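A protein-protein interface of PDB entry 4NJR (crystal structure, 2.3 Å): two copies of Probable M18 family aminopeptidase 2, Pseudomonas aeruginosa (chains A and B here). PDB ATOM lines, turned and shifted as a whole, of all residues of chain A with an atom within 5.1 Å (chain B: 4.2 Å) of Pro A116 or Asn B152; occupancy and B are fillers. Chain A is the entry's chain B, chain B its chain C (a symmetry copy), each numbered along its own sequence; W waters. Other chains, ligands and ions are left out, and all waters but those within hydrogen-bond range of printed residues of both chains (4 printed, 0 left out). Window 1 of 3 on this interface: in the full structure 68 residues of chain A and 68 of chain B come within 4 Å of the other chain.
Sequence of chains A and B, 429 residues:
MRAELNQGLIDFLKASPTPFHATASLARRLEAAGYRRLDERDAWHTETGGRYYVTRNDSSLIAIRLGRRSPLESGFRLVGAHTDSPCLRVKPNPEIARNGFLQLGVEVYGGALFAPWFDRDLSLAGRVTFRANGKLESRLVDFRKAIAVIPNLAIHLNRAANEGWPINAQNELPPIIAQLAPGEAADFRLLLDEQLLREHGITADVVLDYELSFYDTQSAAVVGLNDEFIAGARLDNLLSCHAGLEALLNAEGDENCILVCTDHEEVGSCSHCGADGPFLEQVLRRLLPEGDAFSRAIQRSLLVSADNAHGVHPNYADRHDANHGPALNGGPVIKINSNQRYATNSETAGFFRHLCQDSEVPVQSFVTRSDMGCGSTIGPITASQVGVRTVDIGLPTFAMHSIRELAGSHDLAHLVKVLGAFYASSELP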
ATOM      1  N   LEU A 113      11.313  12.497 -15.508  1.00  0.00           N
ATOM      2  CA  LEU A 113      11.046  13.496 -14.477  1.00  0.00           C
ATOM      3  C   LEU A 113      12.378  14.062 -14.002  1.00  0.00           C
ATOM      4  O   LEU A 113      13.191  13.306 -13.528  1.00  0.00           O
ATOM      5  CB  LEU A 113      10.329  12.871 -13.298  1.00  0.00           C
ATOM      6  CG  LEU A 113       8.853  12.590 -13.493  1.00  0.00           C
ATOM      7  CD1 LEU A 113       8.291  11.992 -12.193  1.00  0.00           C
ATOM      8  CD2 LEU A 113       8.177  13.893 -13.813  1.00  0.00           C
ATOM      9  N   PHE A 114      12.630  15.353 -14.202  1.00  0.00           N
ATOM     10  CA  PHE A 114      13.919  15.944 -13.833  1.00  0.00           C
ATOM     11  C   PHE A 114      14.135  15.983 -12.329  1.00  0.00           C
ATOM     12  O   PHE A 114      15.229  15.651 -11.834  1.00  0.00           O
ATOM     13  CB  PHE A 114      14.125  17.377 -14.400  1.00  0.00           C
ATOM     14  CG  PHE A 114      14.037  17.483 -15.931  1.00  0.00           C
ATOM     15  CD1 PHE A 114      14.020  16.362 -16.734  1.00  0.00           C
ATOM     16  CD2 PHE A 114      13.962  18.735 -16.552  1.00  0.00           C
ATOM     17  CE1 PHE A 114      13.933  16.475 -18.137  1.00  0.00           C
ATOM     18  CE2 PHE A 114      13.885  18.843 -17.954  1.00  0.00           C
ATOM     19  CZ  PHE A 114      13.840  17.694 -18.754  1.00  0.00           C
ATOM     20  N   ALA A 115      13.121  16.400 -11.580  1.00  0.00           N
ATOM     21  CA  ALA A 115      13.403  16.788 -10.193  1.00  0.00           C
ATOM     22  C   ALA A 115      13.999  15.618  -9.356  1.00  0.00           C
ATOM     23  O   ALA A 115      14.909  15.805  -8.544  1.00  0.00           O
ATOM     24  CB  ALA A 115      12.151  17.407  -9.534  1.00  0.00           C
ATOM     25  N   PRO A 116      13.473  14.397  -9.552  1.00  0.00           N
ATOM     26  CA  PRO A 116      14.019  13.300  -8.758  1.00  0.00           C
ATOM     27  C   PRO A 116      15.493  12.967  -9.016  1.00  0.00           C
ATOM     28  O   PRO A 116      16.088  12.290  -8.210  1.00  0.00           O
ATOM     29  CB  PRO A 116      13.142  12.114  -9.133  1.00  0.00           C
ATOM     30  CG  PRO A 116      11.921  12.715  -9.748  1.00  0.00           C
ATOM     31  CD  PRO A 116      12.321  14.004 -10.352  1.00  0.00           C
ATOM     32  N   TRP A 117      16.063  13.403 -10.145  1.00  0.00           N
ATOM     33  CA  TRP A 117      17.491  13.219 -10.407  1.00  0.00           C
ATOM     34  C   TRP A 117      18.408  14.016  -9.510  1.00  0.00           C
ATOM     35  O   TRP A 117      19.622  13.703  -9.367  1.00  0.00           O
ATOM     36  CB  TRP A 117      17.795  13.445 -11.888  1.00  0.00           C
ATOM     37  CG  TRP A 117      17.357  12.241 -12.677  1.00  0.00           C
ATOM     38  CD1 TRP A 117      16.107  11.944 -13.055  1.00  0.00           C
ATOM     39  CD2 TRP A 117      18.168  11.143 -13.047  1.00  0.00           C
ATOM     40  NE1 TRP A 117      16.064  10.747 -13.662  1.00  0.00           N
ATOM     41  CE2 TRP A 117      17.326  10.200 -13.647  1.00  0.00           C
ATOM     42  CE3 TRP A 117      19.530  10.860 -12.922  1.00  0.00           C
ATOM     43  CZ2 TRP A 117      17.804   8.998 -14.217  1.00  0.00           C
ATOM     44  CZ3 TRP A 117      20.012   9.620 -13.445  1.00  0.00           C
ATOM     45  CH2 TRP A 117      19.120   8.709 -14.078  1.00  0.00           C
ATOM     46  N   PHE A 118      17.852  15.059  -8.882  1.00  0.00           N
ATOM     47  CA  PHE A 118      18.677  15.916  -8.021  1.00  0.00           C
ATOM     48  C   PHE A 118      18.882  15.225  -6.679  1.00  0.00           C
ATOM     49  O   PHE A 118      17.974  14.536  -6.169  1.00  0.00           O
ATOM     50  CB  PHE A 118      18.032  17.267  -7.761  1.00  0.00           C
ATOM     51  CG  PHE A 118      17.967  18.166  -8.932  1.00  0.00           C
ATOM     52  CD1 PHE A 118      17.194  17.858 -10.023  1.00  0.00           C
ATOM     53  CD2 PHE A 118      18.669  19.356  -8.934  1.00  0.00           C
ATOM     54  CE1 PHE A 118      17.098  18.731 -11.088  1.00  0.00           C
ATOM     55  CE2 PHE A 118      18.579  20.229 -10.004  1.00  0.00           C
ATOM     56  CZ  PHE A 118      17.752  19.943 -11.063  1.00  0.00           C
ATOM     57  N   ARG A 120      20.939  12.824  -5.531  1.00  0.00           N
ATOM     58  CA  ARG A 120      21.097  11.398  -5.587  1.00  0.00           C
ATOM     59  C   ARG A 120      22.551  11.096  -5.842  1.00  0.00           C
ATOM     60  O   ARG A 120      23.217  11.870  -6.476  1.00  0.00           O
ATOM     61  CB  ARG A 120      20.284  10.835  -6.749  1.00  0.00           C
ATOM     62  CG  ARG A 120      18.830  11.158  -6.745  1.00  0.00           C
ATOM     63  CD  ARG A 120      18.005  10.336  -5.755  1.00  0.00           C
ATOM     64  NE  ARG A 120      16.599  10.651  -5.880  1.00  0.00           N
ATOM     65  CZ  ARG A 120      15.600   9.971  -5.346  1.00  0.00           C
ATOM     66  NH1 ARG A 120      15.813   8.901  -4.628  1.00  0.00           N
ATOM     67  NH2 ARG A 120      14.362  10.370  -5.555  1.00  0.00           N
ATOM     68  N   HIS A 313      -3.050   6.790  -7.557  1.00  0.00           N
ATOM     69  CA  HIS A 313      -2.227   7.381  -6.520  1.00  0.00           C
ATOM     70  C   HIS A 313      -3.159   8.124  -5.560  1.00  0.00           C
ATOM     71  O   HIS A 313      -3.909   9.028  -5.956  1.00  0.00           O
ATOM     72  CB  HIS A 313      -1.251   8.356  -7.215  1.00  0.00           C
ATOM     73  CG  HIS A 313      -0.047   8.777  -6.412  1.00  0.00           C
ATOM     74  ND1 HIS A 313      -0.113   9.139  -5.087  1.00  0.00           N
ATOM     75  CD2 HIS A 313       1.252   8.939  -6.784  1.00  0.00           C
ATOM     76  CE1 HIS A 313       1.088   9.509  -4.681  1.00  0.00           C
ATOM     77  NE2 HIS A 313       1.937   9.380  -5.685  1.00  0.00           N
ATOM     78  N   TYR A 316      -3.157  11.821  -5.646  1.00  0.00           N
ATOM     79  CA  TYR A 316      -3.495  12.374  -6.941  1.00  0.00           C
ATOM     80  C   TYR A 316      -4.573  11.531  -7.626  1.00  0.00           C
ATOM     81  O   TYR A 316      -4.475  11.244  -8.850  1.00  0.00           O
ATOM     82  CB  TYR A 316      -2.275  12.439  -7.924  1.00  0.00           C
ATOM     83  CG  TYR A 316      -1.045  13.165  -7.452  1.00  0.00           C
ATOM     84  CD1 TYR A 316      -0.927  14.514  -7.614  1.00  0.00           C
ATOM     85  CD2 TYR A 316       0.030  12.474  -6.884  1.00  0.00           C
ATOM     86  CE1 TYR A 316       0.206  15.170  -7.212  1.00  0.00           C
ATOM     87  CE2 TYR A 316       1.152  13.128  -6.447  1.00  0.00           C
ATOM     88  CZ  TYR A 316       1.252  14.463  -6.616  1.00  0.00           C
ATOM     89  OH  TYR A 316       2.362  15.156  -6.187  1.00  0.00           O
ATOM     90  N   PHE A 398       3.711   3.436  -9.384  1.00  0.00           N
ATOM     91  CA  PHE A 398       3.684   4.878  -9.257  1.00  0.00           C
ATOM     92  C   PHE A 398       5.002   5.507  -9.695  1.00  0.00           C
ATOM     93  O   PHE A 398       6.069   4.869  -9.690  1.00  0.00           O
ATOM     94  CB  PHE A 398       3.513   5.283  -7.800  1.00  0.00           C
ATOM     95  CG  PHE A 398       2.243   4.851  -7.162  1.00  0.00           C
ATOM     96  CD1 PHE A 398       1.018   4.907  -7.850  1.00  0.00           C
ATOM     97  CD2 PHE A 398       2.243   4.510  -5.817  1.00  0.00           C
ATOM     98  CE1 PHE A 398      -0.142   4.578  -7.209  1.00  0.00           C
ATOM     99  CE2 PHE A 398       1.056   4.176  -5.158  1.00  0.00           C
ATOM    100  CZ  PHE A 398      -0.143   4.187  -5.859  1.00  0.00           C
ATOM    101  N   ALA A 399       4.929   6.803  -9.965  1.00  0.00           N
ATOM    102  CA  ALA A 399       6.111   7.644 -10.135  1.00  0.00           C
ATOM    103  C   ALA A 399       6.904   7.290 -11.357  1.00  0.00           C
ATOM    104  O   ALA A 399       8.158   7.427 -11.422  1.00  0.00           O
ATOM    105  CB  ALA A 399       6.992   7.627  -8.897  1.00  0.00           C
ATOM    106  N   SER A 402      10.384   8.579 -12.826  1.00  0.00           N
ATOM    107  CA  SER A 402      11.281   9.020 -11.802  1.00  0.00           C
ATOM    108  C   SER A 402      12.598   8.225 -11.860  1.00  0.00           C
ATOM    109  O   SER A 402      12.666   7.174 -12.474  1.00  0.00           O
ATOM    110  CB  SER A 402      10.610   8.894 -10.416  1.00  0.00           C
ATOM    111  OG  SER A 402      11.543   9.189  -9.347  1.00  0.00           O
ATOM    112  N   ILE A 403      13.616   8.700 -11.139  1.00  0.00           N
ATOM    113  CA  ILE A 403      14.765   7.889 -10.790  1.00  0.00           C
ATOM    114  C   ILE A 403      14.469   6.765  -9.818  1.00  0.00           C
ATOM    115  O   ILE A 403      15.313   5.853  -9.620  1.00  0.00           O
ATOM    116  CB  ILE A 403      15.914   8.795 -10.259  1.00  0.00           C
ATOM    117  CG1 ILE A 403      17.240   8.171 -10.516  1.00  0.00           C
ATOM    118  CG2 ILE A 403      15.764   9.154  -8.802  1.00  0.00           C
ATOM    119  CD1 ILE A 403      18.416   9.010 -10.079  1.00  0.00           C
ATOM    120  N   PHE B 118      10.176  13.278  -2.297  1.00  0.00           N
ATOM    121  CA  PHE B 118       9.461  12.310  -3.091  1.00  0.00           C
ATOM    122  C   PHE B 118      10.405  11.208  -3.532  1.00  0.00           C
ATOM    123  O   PHE B 118      11.556  11.474  -3.830  1.00  0.00           O
ATOM    124  CB  PHE B 118       8.854  12.949  -4.326  1.00  0.00           C
ATOM    125  CG  PHE B 118       7.655  13.811  -4.067  1.00  0.00           C
ATOM    126  CD1 PHE B 118       7.785  15.066  -3.512  1.00  0.00           C
ATOM    127  CD2 PHE B 118       6.406  13.430  -4.496  1.00  0.00           C
ATOM    128  CE1 PHE B 118       6.688  15.928  -3.368  1.00  0.00           C
ATOM    129  CE2 PHE B 118       5.322  14.276  -4.328  1.00  0.00           C
ATOM    130  CZ  PHE B 118       5.470  15.543  -3.811  1.00  0.00           C
ATOM    131  N   ASP B 119       9.863   9.996  -3.612  1.00  0.00           N
ATOM    132  CA  ASP B 119      10.564   8.845  -4.174  1.00  0.00           C
ATOM    133  C   ASP B 119      11.868   8.552  -3.401  1.00  0.00           C
ATOM    134  O   ASP B 119      12.946   8.366  -3.965  1.00  0.00           O
ATOM    135  CB  ASP B 119      10.835   9.062  -5.648  1.00  0.00           C
ATOM    136  CG  ASP B 119       9.602   9.348  -6.425  1.00  0.00           C
ATOM    137  OD1 ASP B 119       8.473   8.936  -5.964  1.00  0.00           O
ATOM    138  OD2 ASP B 119       9.779   9.900  -7.561  1.00  0.00           O
ATOM    139  N   ILE B 150       6.665   8.680  -0.309  1.00  0.00           N
ATOM    140  CA  ILE B 150       5.872   9.717  -0.928  1.00  0.00           C
ATOM    141  C   ILE B 150       6.111   9.668  -2.467  1.00  0.00           C
ATOM    142  O   ILE B 150       7.029  10.259  -3.006  1.00  0.00           O
ATOM    143  CB  ILE B 150       6.224  11.125  -0.367  1.00  0.00           C
ATOM    144  CG1 ILE B 150       5.973  11.192   1.124  1.00  0.00           C
ATOM    145  CG2 ILE B 150       5.395  12.212  -1.059  1.00  0.00           C
ATOM    146  CD1 ILE B 150       6.873  12.222   1.764  1.00  0.00           C
ATOM    147  N   PRO B 151       5.297   8.925  -3.187  1.00  0.00           N
ATOM    148  CA  PRO B 151       5.656   8.743  -4.608  1.00  0.00           C
ATOM    149  C   PRO B 151       5.295   9.940  -5.462  1.00  0.00           C
ATOM    150  O   PRO B 151       4.229  10.546  -5.239  1.00  0.00           O
ATOM    151  CB  PRO B 151       4.770   7.565  -5.047  1.00  0.00           C
ATOM    152  CG  PRO B 151       4.100   7.042  -3.790  1.00  0.00           C
ATOM    153  CD  PRO B 151       4.072   8.205  -2.843  1.00  0.00           C
ATOM    154  N   ASN B 152       6.135  10.231  -6.464  1.00  0.00           N
ATOM    155  CA  ASN B 152       5.763  11.175  -7.493  1.00  0.00           C
ATOM    156  C   ASN B 152       4.582  10.629  -8.271  1.00  0.00           C
ATOM    157  O   ASN B 152       4.318   9.454  -8.215  1.00  0.00           O
ATOM    158  CB  ASN B 152       6.914  11.559  -8.394  1.00  0.00           C
ATOM    159  CG  ASN B 152       7.619  12.823  -7.928  1.00  0.00           C
ATOM    160  OD1 ASN B 152       7.045  13.930  -7.854  1.00  0.00           O
ATOM    161  ND2 ASN B 152       8.860  12.680  -7.625  1.00  0.00           N
ATOM    162  N   LEU B 153       3.840  11.530  -8.894  1.00  0.00           N
ATOM    163  CA  LEU B 153       2.835  11.209  -9.911  1.00  0.00           C
ATOM    164  C   LEU B 153       3.592  11.012 -11.200  1.00  0.00           C
ATOM    165  O   LEU B 153       4.416  11.849 -11.550  1.00  0.00           O
ATOM    166  CB  LEU B 153       1.842  12.381 -10.098  1.00  0.00           C
ATOM    167  CG  LEU B 153       0.773  12.178 -11.192  1.00  0.00           C
ATOM    168  CD1 LEU B 153      -0.081  10.924 -10.956  1.00  0.00           C
ATOM    169  CD2 LEU B 153      -0.089  13.445 -11.344  1.00  0.00           C
ATOM    170  N   ALA B 154       3.268   9.941 -11.927  1.00  0.00           N
ATOM    171  CA  ALA B 154       3.924   9.682 -13.207  1.00  0.00           C
ATOM    172  C   ALA B 154       3.893  10.902 -14.092  1.00  0.00           C
ATOM    173  O   ALA B 154       2.888  11.580 -14.186  1.00  0.00           O
ATOM    174  CB  ALA B 154       3.264   8.516 -13.963  1.00  0.00           C
HETATM  175  O   HOH W   1       4.504  14.473  -8.122  1.00  0.00           O
HETATM  176  O   HOH W   2       2.693  11.881  -3.370  1.00  0.00           O
HETATM  177  O   HOH W   3      13.011  13.171  -5.477  1.00  0.00           O
HETATM  178  O   HOH W   4       1.897   7.601 -10.736  1.00  0.00           O
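O of Phe B118 is in hydrogen-bond range of NH2 of Arg A120 (3.5 Å).
The guanidinium group (NH2) of Arg A120 is in hydrogen-bond range of the backbone carbonyl oxygen (O) of Asp B119.
O of Pro B151 sits at hydrogen-bond distance from NE2 of His A313 (2.6 Å).
A ring nitrogen (NE2) of His A313 sits close to the backbone carbonyl oxygen (O) of Asn B152, at 3.5 Å.
N of Ala A399 lies close to O of Asn B152, at 3.2 Å.
The side-chain hydroxyl of Ser A402 is in hydrogen-bond range of the side-chain carboxylate of Asp B119, 2.6 Å away.
The backbone carbonyl oxygen of Pro A116 lies within hydrogen-bond range of the guanidinium group of Arg A120, at 2.9 Å.
N of Asp B119 is in hydrogen-bond range of O of Ile B150, 2.9 Å away.
OD1 of Asp B119 sits at hydrogen-bond distance from N of Asn B152, 2.7 Å away.
Among the printed residues, pairs that only touch across the chains: Ala A399 with Asp B119, Tyr A316 with Phe B118, Tyr A316 with Leu B153, Pro A116 with Asn B152, Phe A398 with Pro B151 and Leu A113 with Leu B153.
Phe A114 touches none of the printed residues of chain B.
Ala A115 touches none of the printed residues of chain B.
Pro A116 touches one residue of chain B.
Of the printed residues of chain B, Arg A120 touches Phe B118 and Asp B119.
Of the printed residues of chain B, Tyr A316 touches Phe B118 and Leu B153.
Of the printed residues of chain B, Phe A398 touches Pro B151 (3.7 Å).
Printed residues of chain A within 4 Å of Asp B119: Arg A120, Ala A399 and Ser A402.
Asn B152 touches three residues of chain A.
The nearest residue of chain A that does not touch Asn B152 is Leu A113 (4.1 Å).
The nearest printed residue of chain B that does not touch Ser A402 is Asn B152 (4.7 Å).
Hydrophobic or aromatic side chains of chain A within 4 Å of the printed part of chain B: Leu A113, Pro A116, His A313, Tyr A316, Phe A398 and Ala A399.
Along chain A the printed residues that touch a printed residue of chain B span positions 113 to 402.
Hydrophobic or aromatic side chains of chain B within 4 Å of the printed part of chain A: Phe B118, Pro B151 and Leu B153.
Among the printed residues, no Asp or Glu carboxylate lies within 4 Å of a Lys or Arg side-chain nitrogen of the other chain.
Position printed for both chains: 118.
Of the 12 pairs that touch across the chains among the printed residues, none has its exchanged pair printed and touching as well.
Water W1 lies within hydrogen-bond range of OD1 of Asn B152, OH of Tyr A316 and N of Leu B153.
Water W2 lies within hydrogen-bond range of O of Pro B151 (2.8 Å) and NE2 of His A313 (3.5 Å).
Water W3 bridges the backbone carbonyl oxygen (O) of Phe B118 (2.8 Å) and the guanidinium group (NH2) of Arg A120 (3.1 Å).
Water W4 bridges the backbone NH (N) of Ala B154 (3.0 Å) and the backbone NH (N) of Ala A399 (3.2 Å).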
